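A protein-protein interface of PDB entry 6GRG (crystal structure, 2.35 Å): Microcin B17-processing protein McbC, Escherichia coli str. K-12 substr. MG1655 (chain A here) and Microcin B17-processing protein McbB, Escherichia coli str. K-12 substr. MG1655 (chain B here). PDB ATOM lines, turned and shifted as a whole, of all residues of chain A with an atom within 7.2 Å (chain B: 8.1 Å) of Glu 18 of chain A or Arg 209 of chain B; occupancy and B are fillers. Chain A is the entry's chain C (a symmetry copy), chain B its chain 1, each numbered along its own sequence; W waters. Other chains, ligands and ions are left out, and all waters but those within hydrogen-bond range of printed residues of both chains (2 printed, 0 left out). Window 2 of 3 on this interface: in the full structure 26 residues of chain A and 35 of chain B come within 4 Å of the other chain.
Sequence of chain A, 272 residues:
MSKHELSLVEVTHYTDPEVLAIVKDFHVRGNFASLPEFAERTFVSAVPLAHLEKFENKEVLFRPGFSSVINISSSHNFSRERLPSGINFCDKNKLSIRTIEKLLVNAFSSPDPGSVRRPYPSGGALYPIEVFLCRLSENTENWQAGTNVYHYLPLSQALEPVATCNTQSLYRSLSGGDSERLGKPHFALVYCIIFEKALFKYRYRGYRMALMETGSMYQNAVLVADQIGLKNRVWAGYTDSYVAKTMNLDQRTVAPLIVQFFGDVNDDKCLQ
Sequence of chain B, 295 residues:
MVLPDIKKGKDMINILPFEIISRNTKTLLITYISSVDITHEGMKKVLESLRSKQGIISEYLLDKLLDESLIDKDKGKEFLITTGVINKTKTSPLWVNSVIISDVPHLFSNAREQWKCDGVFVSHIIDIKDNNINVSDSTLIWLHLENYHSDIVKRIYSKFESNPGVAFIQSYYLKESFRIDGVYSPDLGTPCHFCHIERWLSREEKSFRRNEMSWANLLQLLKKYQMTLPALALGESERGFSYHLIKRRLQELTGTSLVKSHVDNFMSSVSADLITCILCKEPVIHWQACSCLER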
ATOM      1  N   THR A  15      -0.568   0.582  16.972  1.00  0.00           N
ATOM      2  CA  THR A  15       0.616   0.873  16.166  1.00  0.00           C
ATOM      3  C   THR A  15       1.828   0.102  16.719  1.00  0.00           C
ATOM      4  O   THR A  15       2.128   0.104  17.913  1.00  0.00           O
ATOM      5  CB  THR A  15       0.888   2.383  16.071  1.00  0.00           C
ATOM      6  OG1 THR A  15      -0.089   2.929  15.191  1.00  0.00           O
ATOM      7  CG2 THR A  15       2.271   2.741  15.555  1.00  0.00           C
ATOM      8  N   ASP A  16       2.515  -0.598  15.812  1.00  0.00           N
ATOM      9  CA  ASP A  16       3.844  -1.088  16.058  1.00  0.00           C
ATOM     10  C   ASP A  16       4.809   0.059  15.745  1.00  0.00           C
ATOM     11  O   ASP A  16       4.942   0.515  14.603  1.00  0.00           O
ATOM     12  CB  ASP A  16       4.090  -2.375  15.271  1.00  0.00           C
ATOM     13  CG  ASP A  16       5.444  -2.981  15.577  1.00  0.00           C
ATOM     14  OD1 ASP A  16       6.321  -2.266  16.143  1.00  0.00           O
ATOM     15  OD2 ASP A  16       5.604  -4.165  15.281  1.00  0.00           O
ATOM     16  N   PRO A  17       5.534   0.589  16.743  1.00  0.00           N
ATOM     17  CA  PRO A  17       6.416   1.732  16.492  1.00  0.00           C
ATOM     18  C   PRO A  17       7.652   1.395  15.628  1.00  0.00           C
ATOM     19  O   PRO A  17       8.182   2.260  14.950  1.00  0.00           O
ATOM     20  CB  PRO A  17       6.837   2.124  17.915  1.00  0.00           C
ATOM     21  CG  PRO A  17       6.845   0.809  18.653  1.00  0.00           C
ATOM     22  CD  PRO A  17       5.639   0.070  18.113  1.00  0.00           C
ATOM     23  N   GLU A  18       8.134   0.155  15.709  1.00  0.00           N
ATOM     24  CA  GLU A  18       9.175  -0.334  14.821  1.00  0.00           C
ATOM     25  C   GLU A  18       8.715  -0.206  13.354  1.00  0.00           C
ATOM     26  O   GLU A  18       9.444   0.292  12.478  1.00  0.00           O
ATOM     27  CB  GLU A  18       9.508  -1.779  15.193  1.00  0.00           C
ATOM     28  CG  GLU A  18      10.686  -2.352  14.427  1.00  0.00           C
ATOM     29  CD  GLU A  18      12.062  -1.918  14.919  1.00  0.00           C
ATOM     30  OE1 GLU A  18      12.130  -1.127  15.906  1.00  0.00           O
ATOM     31  OE2 GLU A  18      13.072  -2.381  14.324  1.00  0.00           O
ATOM     32  N   VAL A  19       7.490  -0.654  13.073  1.00  0.00           N
ATOM     33  CA  VAL A  19       6.987  -0.683  11.714  1.00  0.00           C
ATOM     34  C   VAL A  19       6.898   0.753  11.177  1.00  0.00           C
ATOM     35  O   VAL A  19       7.285   1.024  10.066  1.00  0.00           O
ATOM     36  CB  VAL A  19       5.630  -1.407  11.631  1.00  0.00           C
ATOM     37  CG1 VAL A  19       4.986  -1.219  10.273  1.00  0.00           C
ATOM     38  CG2 VAL A  19       5.764  -2.879  11.938  1.00  0.00           C
ATOM     39  N   LEU A  20       6.388   1.664  12.006  1.00  0.00           N
ATOM     40  CA  LEU A  20       6.136   3.032  11.644  1.00  0.00           C
ATOM     41  C   LEU A  20       7.442   3.743  11.329  1.00  0.00           C
ATOM     42  O   LEU A  20       7.518   4.514  10.391  1.00  0.00           O
ATOM     43  CB  LEU A  20       5.434   3.713  12.817  1.00  0.00           C
ATOM     44  CG  LEU A  20       5.081   5.177  12.589  1.00  0.00           C
ATOM     45  CD1 LEU A  20       4.003   5.319  11.513  1.00  0.00           C
ATOM     46  CD2 LEU A  20       4.643   5.814  13.890  1.00  0.00           C
ATOM     47  N   ALA A  21       8.453   3.502  12.165  1.00  0.00           N
ATOM     48  CA  ALA A  21       9.779   4.087  11.971  1.00  0.00           C
ATOM     49  C   ALA A  21      10.432   3.590  10.688  1.00  0.00           C
ATOM     50  O   ALA A  21      11.034   4.397  10.014  1.00  0.00           O
ATOM     51  CB  ALA A  21      10.683   3.752  13.109  1.00  0.00           C
ATOM     52  N   ILE A  22      10.372   2.272  10.419  1.00  0.00           N
ATOM     53  CA  ILE A  22      11.024   1.671   9.230  1.00  0.00           C
ATOM     54  C   ILE A  22      10.325   2.158   7.935  1.00  0.00           C
ATOM     55  O   ILE A  22      10.990   2.461   6.917  1.00  0.00           O
ATOM     56  CB  ILE A  22      11.093   0.131   9.374  1.00  0.00           C
ATOM     57  CG1 ILE A  22      12.140  -0.237  10.426  1.00  0.00           C
ATOM     58  CG2 ILE A  22      11.357  -0.568   8.048  1.00  0.00           C
ATOM     59  CD1 ILE A  22      12.071  -1.652  10.884  1.00  0.00           C
ATOM     60  N   VAL A  23       8.993   2.289   7.970  1.00  0.00           N
ATOM     61  CA  VAL A  23       8.204   2.751   6.810  1.00  0.00           C
ATOM     62  C   VAL A  23       8.494   4.237   6.521  1.00  0.00           C
ATOM     63  O   VAL A  23       8.615   4.641   5.353  1.00  0.00           O
ATOM     64  CB  VAL A  23       6.697   2.537   7.042  1.00  0.00           C
ATOM     65  CG1 VAL A  23       5.859   3.184   5.939  1.00  0.00           C
ATOM     66  CG2 VAL A  23       6.365   1.074   7.176  1.00  0.00           C
ATOM     67  N   LYS A  24       8.543   5.070   7.565  1.00  0.00           N
ATOM     68  CA  LYS A  24       8.798   6.491   7.370  1.00  0.00           C
ATOM     69  C   LYS A  24      10.238   6.701   6.888  1.00  0.00           C
ATOM     70  O   LYS A  24      10.458   7.515   5.996  1.00  0.00           O
ATOM     71  CB  LYS A  24       8.595   7.296   8.653  1.00  0.00           C
ATOM     72  CG  LYS A  24       7.168   7.473   9.148  1.00  0.00           C
ATOM     73  CD  LYS A  24       7.195   7.865  10.628  1.00  0.00           C
ATOM     74  CE  LYS A  24       5.985   8.636  11.107  1.00  0.00           C
ATOM     75  NZ  LYS A  24       6.359   9.691  12.091  1.00  0.00           N
ATOM     76  N   ASP A  25      11.213   6.003   7.497  1.00  0.00           N
ATOM     77  CA  ASP A  25      12.623   6.040   7.042  1.00  0.00           C
ATOM     78  C   ASP A  25      12.705   5.774   5.535  1.00  0.00           C
ATOM     79  O   ASP A  25      13.432   6.464   4.811  1.00  0.00           O
ATOM     80  CB  ASP A  25      13.479   4.960   7.682  1.00  0.00           C
ATOM     81  CG  ASP A  25      13.840   5.233   9.119  1.00  0.00           C
ATOM     82  OD1 ASP A  25      13.624   6.386   9.592  1.00  0.00           O
ATOM     83  OD2 ASP A  25      14.338   4.277   9.759  1.00  0.00           O
ATOM     84  N   ARG A 203       0.244  -3.960   8.920  1.00  0.00           N
ATOM     85  CA  ARG A 203       1.670  -3.693   9.075  1.00  0.00           C
ATOM     86  C   ARG A 203       2.223  -3.291   7.699  1.00  0.00           C
ATOM     87  O   ARG A 203       1.532  -2.639   6.941  1.00  0.00           O
ATOM     88  CB  ARG A 203       2.370  -4.911   9.679  1.00  0.00           C
ATOM     89  CG  ARG A 203       1.800  -5.397  10.999  1.00  0.00           C
ATOM     90  CD  ARG A 203       2.419  -6.704  11.478  1.00  0.00           C
ATOM     91  NE  ARG A 203       3.883  -6.734  11.529  1.00  0.00           N
ATOM     92  CZ  ARG A 203       4.616  -6.208  12.497  1.00  0.00           C
ATOM     93  NH1 ARG A 203       4.035  -5.651  13.549  1.00  0.00           N
ATOM     94  NH2 ARG A 203       5.929  -6.229  12.398  1.00  0.00           N
ATOM     95  N   TYR A 204       3.437  -3.734   7.348  1.00  0.00           N
ATOM     96  CA  TYR A 204       4.194  -3.159   6.218  1.00  0.00           C
ATOM     97  C   TYR A 204       3.403  -3.223   4.908  1.00  0.00           C
ATOM     98  O   TYR A 204       3.390  -2.261   4.150  1.00  0.00           O
ATOM     99  CB  TYR A 204       5.502  -3.908   6.047  1.00  0.00           C
ATOM    100  CG  TYR A 204       6.499  -3.696   7.155  1.00  0.00           C
ATOM    101  CD1 TYR A 204       7.306  -2.573   7.145  1.00  0.00           C
ATOM    102  CD2 TYR A 204       6.728  -4.664   8.129  1.00  0.00           C
ATOM    103  CE1 TYR A 204       8.254  -2.367   8.133  1.00  0.00           C
ATOM    104  CE2 TYR A 204       7.689  -4.484   9.119  1.00  0.00           C
ATOM    105  CZ  TYR A 204       8.437  -3.321   9.118  1.00  0.00           C
ATOM    106  OH  TYR A 204       9.374  -3.054  10.047  1.00  0.00           O
ATOM    107  N   ARG B 199      18.145  10.628  15.802  1.00  0.00           N
ATOM    108  CA  ARG B 199      18.272   9.535  14.833  1.00  0.00           C
ATOM    109  C   ARG B 199      19.600   8.796  15.043  1.00  0.00           C
ATOM    110  O   ARG B 199      19.614   7.567  15.004  1.00  0.00           O
ATOM    111  CB  ARG B 199      18.185  10.034  13.387  1.00  0.00           C
ATOM    112  CG  ARG B 199      18.306   8.918  12.354  1.00  0.00           C
ATOM    113  CD  ARG B 199      17.129   7.959  12.445  1.00  0.00           C
ATOM    114  NE  ARG B 199      17.070   6.923  11.417  1.00  0.00           N
ATOM    115  CZ  ARG B 199      17.640   5.714  11.489  1.00  0.00           C
ATOM    116  NH1 ARG B 199      18.334   5.340  12.557  1.00  0.00           N
ATOM    117  NH2 ARG B 199      17.523   4.886  10.466  1.00  0.00           N
ATOM    118  N   SER B 202      19.786   6.947  18.542  1.00  0.00           N
ATOM    119  CA  SER B 202      19.021   5.720  18.377  1.00  0.00           C
ATOM    120  C   SER B 202      19.860   4.623  17.704  1.00  0.00           C
ATOM    121  O   SER B 202      20.004   3.557  18.242  1.00  0.00           O
ATOM    122  CB  SER B 202      17.762   5.953  17.600  1.00  0.00           C
ATOM    123  OG  SER B 202      17.167   4.712  17.235  1.00  0.00           O
ATOM    124  N   ARG B 203      20.407   4.890  16.518  1.00  0.00           N
ATOM    125  CA  ARG B 203      21.242   3.914  15.809  1.00  0.00           C
ATOM    126  C   ARG B 203      22.415   3.429  16.692  1.00  0.00           C
ATOM    127  O   ARG B 203      22.816   2.258  16.616  1.00  0.00           O
ATOM    128  CB  ARG B 203      21.717   4.527  14.489  1.00  0.00           C
ATOM    129  CG  ARG B 203      22.614   3.615  13.664  1.00  0.00           C
ATOM    130  CD  ARG B 203      22.934   4.184  12.289  1.00  0.00           C
ATOM    131  NE  ARG B 203      21.806   4.111  11.370  1.00  0.00           N
ATOM    132  CZ  ARG B 203      21.589   4.970  10.379  1.00  0.00           C
ATOM    133  NH1 ARG B 203      22.507   5.875  10.089  1.00  0.00           N
ATOM    134  NH2 ARG B 203      20.449   4.941   9.705  1.00  0.00           N
ATOM    135  N   GLU B 204      22.977   4.296  17.542  1.00  0.00           N
ATOM    136  CA  GLU B 204      24.171   3.922  18.301  1.00  0.00           C
ATOM    137  C   GLU B 204      23.827   2.958  19.465  1.00  0.00           C
ATOM    138  O   GLU B 204      24.697   2.230  19.931  1.00  0.00           O
ATOM    139  CB  GLU B 204      24.893   5.184  18.771  1.00  0.00           C
ATOM    140  CG  GLU B 204      25.535   5.980  17.645  1.00  0.00           C
ATOM    141  CD  GLU B 204      26.830   5.401  17.098  1.00  0.00           C
ATOM    142  OE1 GLU B 204      27.649   4.916  17.900  1.00  0.00           O
ATOM    143  OE2 GLU B 204      27.007   5.414  15.873  1.00  0.00           O
ATOM    144  N   GLU B 205      22.582   2.951  19.965  1.00  0.00           N
ATOM    145  CA  GLU B 205      22.160   1.975  20.997  1.00  0.00           C
ATOM    146  C   GLU B 205      22.320   0.553  20.418  1.00  0.00           C
ATOM    147  O   GLU B 205      21.897   0.318  19.289  1.00  0.00           O
ATOM    148  CB  GLU B 205      20.715   2.244  21.444  1.00  0.00           C
ATOM    149  CG  GLU B 205      20.552   3.408  22.415  1.00  0.00           C
ATOM    150  N   LYS B 206      22.965  -0.371  21.162  1.00  0.00           N
ATOM    151  CA  LYS B 206      23.103  -1.811  20.762  1.00  0.00           C
ATOM    152  C   LYS B 206      21.772  -2.496  21.099  1.00  0.00           C
ATOM    153  O   LYS B 206      21.675  -3.286  22.034  1.00  0.00           O
ATOM    154  CB  LYS B 206      24.319  -2.484  21.423  1.00  0.00           C
ATOM    155  N   SER B 207      20.744  -2.116  20.330  1.00  0.00           N
ATOM    156  CA  SER B 207      19.332  -2.374  20.601  1.00  0.00           C
ATOM    157  C   SER B 207      18.791  -3.469  19.675  1.00  0.00           C
ATOM    158  O   SER B 207      17.777  -4.074  19.995  1.00  0.00           O
ATOM    159  CB  SER B 207      18.529  -1.104  20.428  1.00  0.00           C
ATOM    160  N   PHE B 208      19.464  -3.685  18.531  1.00  0.00           N
ATOM    161  CA  PHE B 208      19.005  -4.492  17.339  1.00  0.00           C
ATOM    162  C   PHE B 208      17.561  -4.113  16.949  1.00  0.00           C
ATOM    163  O   PHE B 208      16.773  -4.967  16.529  1.00  0.00           O
ATOM    164  CB  PHE B 208      19.244  -5.996  17.562  1.00  0.00           C
ATOM    165  CG  PHE B 208      20.704  -6.330  17.757  1.00  0.00           C
ATOM    166  CD1 PHE B 208      21.547  -6.493  16.664  1.00  0.00           C
ATOM    167  CD2 PHE B 208      21.257  -6.375  19.034  1.00  0.00           C
ATOM    168  CE1 PHE B 208      22.901  -6.736  16.842  1.00  0.00           C
ATOM    169  CE2 PHE B 208      22.613  -6.611  19.211  1.00  0.00           C
ATOM    170  CZ  PHE B 208      23.430  -6.797  18.112  1.00  0.00           C
ATOM    171  N   ARG B 209      17.253  -2.813  17.067  1.00  0.00           N
ATOM    172  CA  ARG B 209      15.901  -2.231  16.914  1.00  0.00           C
ATOM    173  C   ARG B 209      16.069  -0.784  16.422  1.00  0.00           C
ATOM    174  O   ARG B 209      16.900  -0.031  16.929  1.00  0.00           O
ATOM    175  CB  ARG B 209      15.071  -2.283  18.213  1.00  0.00           C
ATOM    176  CG  ARG B 209      14.361  -3.609  18.476  1.00  0.00           C
ATOM    177  N   ARG B 210      15.302  -0.439  15.384  1.00  0.00           N
ATOM    178  CA  ARG B 210      15.178   0.917  14.883  1.00  0.00           C
ATOM    179  C   ARG B 210      14.423   1.788  15.908  1.00  0.00           C
ATOM    180  O   ARG B 210      14.838   2.926  16.186  1.00  0.00           O
ATOM    181  CB  ARG B 210      14.500   0.897  13.507  1.00  0.00           C
ATOM    182  CG  ARG B 210      13.966   2.249  13.068  1.00  0.00           C
ATOM    183  CD  ARG B 210      15.053   3.285  13.072  1.00  0.00           C
ATOM    184  NE  ARG B 210      14.553   4.517  12.510  1.00  0.00           N
ATOM    185  CZ  ARG B 210      14.456   5.668  13.160  1.00  0.00           C
ATOM    186  NH1 ARG B 210      14.820   5.756  14.433  1.00  0.00           N
ATOM    187  NH2 ARG B 210      13.996   6.722  12.508  1.00  0.00           N
ATOM    188  N   ASN B 211      13.327   1.255  16.460  1.00  0.00           N
ATOM    189  CA  ASN B 211      12.491   1.982  17.407  1.00  0.00           C
ATOM    190  C   ASN B 211      13.277   2.274  18.698  1.00  0.00           C
ATOM    191  O   ASN B 211      13.662   1.362  19.417  1.00  0.00           O
ATOM    192  CB  ASN B 211      11.207   1.219  17.734  1.00  0.00           C
ATOM    193  CG  ASN B 211      10.525   1.781  18.958  1.00  0.00           C
ATOM    194  OD1 ASN B 211      10.207   2.968  19.007  1.00  0.00           O
ATOM    195  ND2 ASN B 211      10.357   0.950  19.968  1.00  0.00           N
ATOM    196  N   GLU B 212      13.432   3.565  19.016  1.00  0.00           N
ATOM    197  CA  GLU B 212      14.268   4.020  20.139  1.00  0.00           C
ATOM    198  C   GLU B 212      13.483   4.043  21.466  1.00  0.00           C
ATOM    199  O   GLU B 212      14.120   4.183  22.506  1.00  0.00           O
ATOM    200  CB  GLU B 212      14.893   5.399  19.875  1.00  0.00           C
ATOM    201  CG  GLU B 212      14.170   6.293  18.866  1.00  0.00           C
ATOM    202  CD  GLU B 212      13.210   7.334  19.424  1.00  0.00           C
ATOM    203  OE1 GLU B 212      13.523   7.907  20.486  1.00  0.00           O
ATOM    204  OE2 GLU B 212      12.158   7.602  18.785  1.00  0.00           O
ATOM    205  N   MET B 213      12.142   3.876  21.443  1.00  0.00           N
ATOM    206  CA  MET B 213      11.253   4.245  22.600  1.00  0.00           C
ATOM    207  C   MET B 213      11.076   3.077  23.590  1.00  0.00           C
ATOM    208  O   MET B 213      10.823   1.947  23.215  1.00  0.00           O
ATOM    209  CB  MET B 213       9.872   4.728  22.136  1.00  0.00           C
ATOM    210  CG  MET B 213       9.836   6.186  21.730  1.00  0.00           C
ATOM    211  SD  MET B 213      10.429   7.325  23.013  1.00  0.00           S
ATOM    212  CE  MET B 213      10.346   8.882  22.126  1.00  0.00           C
HETATM  213  O   HOH W   1      15.309   8.463   9.246  1.00  0.00           O
HETATM  214  O   HOH W   2       9.818   4.428  16.311  1.00  0.00           O
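Pro 17 of chain A touches just one residue of chain B: Asn 211.
Glu 18 of chain A touches just these residues of chain B: Arg 209 (3.8 Å), Arg 210 (3.1 Å) and Asn 211 (2.7 Å).
Lys 24 of chain A touches none of the printed residues of chain B.
Phe 208 of chain B touches none of the printed residues of chain A.
Arg 209 of chain B touches just one residue of chain A: Glu 18 (3.8 Å).
Of the printed residues of chain A, Arg 210 of chain B touches Glu 18 (3.1 Å), Ala 21 (3.6 Å) and Asp 25 (2.8 Å).
Printed residues of chain A within 4 Å of Asn 211 of chain B: Pro 17 (3.6 Å) and Glu 18 (2.7 Å).
The nearest residue of chain A that does not touch Arg 209 of chain B is Ile 22 of chain A (6.9 Å).
The nearest printed residue of chain B that does not touch Asp 25 of chain A is Arg 203 of chain B (6.1 Å).
Printed residues of chain A that touch a printed residue of chain B: Pro 17, Glu 18, Ala 21 and Asp 25.
Hydrophobic or aromatic side chains of chain A within 4 Å of the printed part of chain B: Pro 17 and Ala 21.
Of the 13 printed residues of chain B, 4 touch a printed residue of chain A.
Printed residues of chain B that touch a printed residue of chain A: Arg 199, Arg 209, Arg 210 and Asn 211.
Among the printed residues, 7 pairs touch across the chains.
Among the printed residues, merely in contact across the chains: Pro 17 of chain A with Asn 211 of chain B, Glu 18 of chain A with Arg 209 of chain B and Ala 21 of chain A with Arg 210 of chain B.
OG of Ser 202 of chain B is in hydrogen-bond range of O of Arg 210 of chain B, at 3.1 Å.
The side-chain amide oxygen (OD1) of Asn 211 of chain B is in hydrogen-bond range of the backbone NH (N) of Met 213 of chain B.
The backbone NH of Glu 18 of chain A sits at hydrogen-bond distance from the side-chain carboxylate of Asp 16 of chain A (3.1 Å).
Water W1 bridges the side-chain carboxylate (OD1) of Asp 25 of chain A (2.7 Å) and the guanidinium group (NE) of Arg 199 of chain B (3.2 Å).
Water W2 bridges the backbone carbonyl oxygen (O) of Pro 17 of chain A (3.0 Å) and the side-chain amide oxygen (OD1) of Asn 211 of chain B (3.1 Å).
The guanidinium group of Arg 199 of chain B is in salt-bridge range of the side-chain carboxylate of Asp 25 of chain A (3.3 Å).
OE2 of Glu 18 of chain A is in hydrogen-bond range of N of Arg 210 of chain B, 3.1 Å away.
The side-chain carboxylate of Asp 25 of chain A is in salt-bridge range of the guanidinium group of Arg 210 of chain B.
N of Asn 211 of chain B lies within hydrogen-bond range of OE1 of Glu 18 of chain A (2.7 Å).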
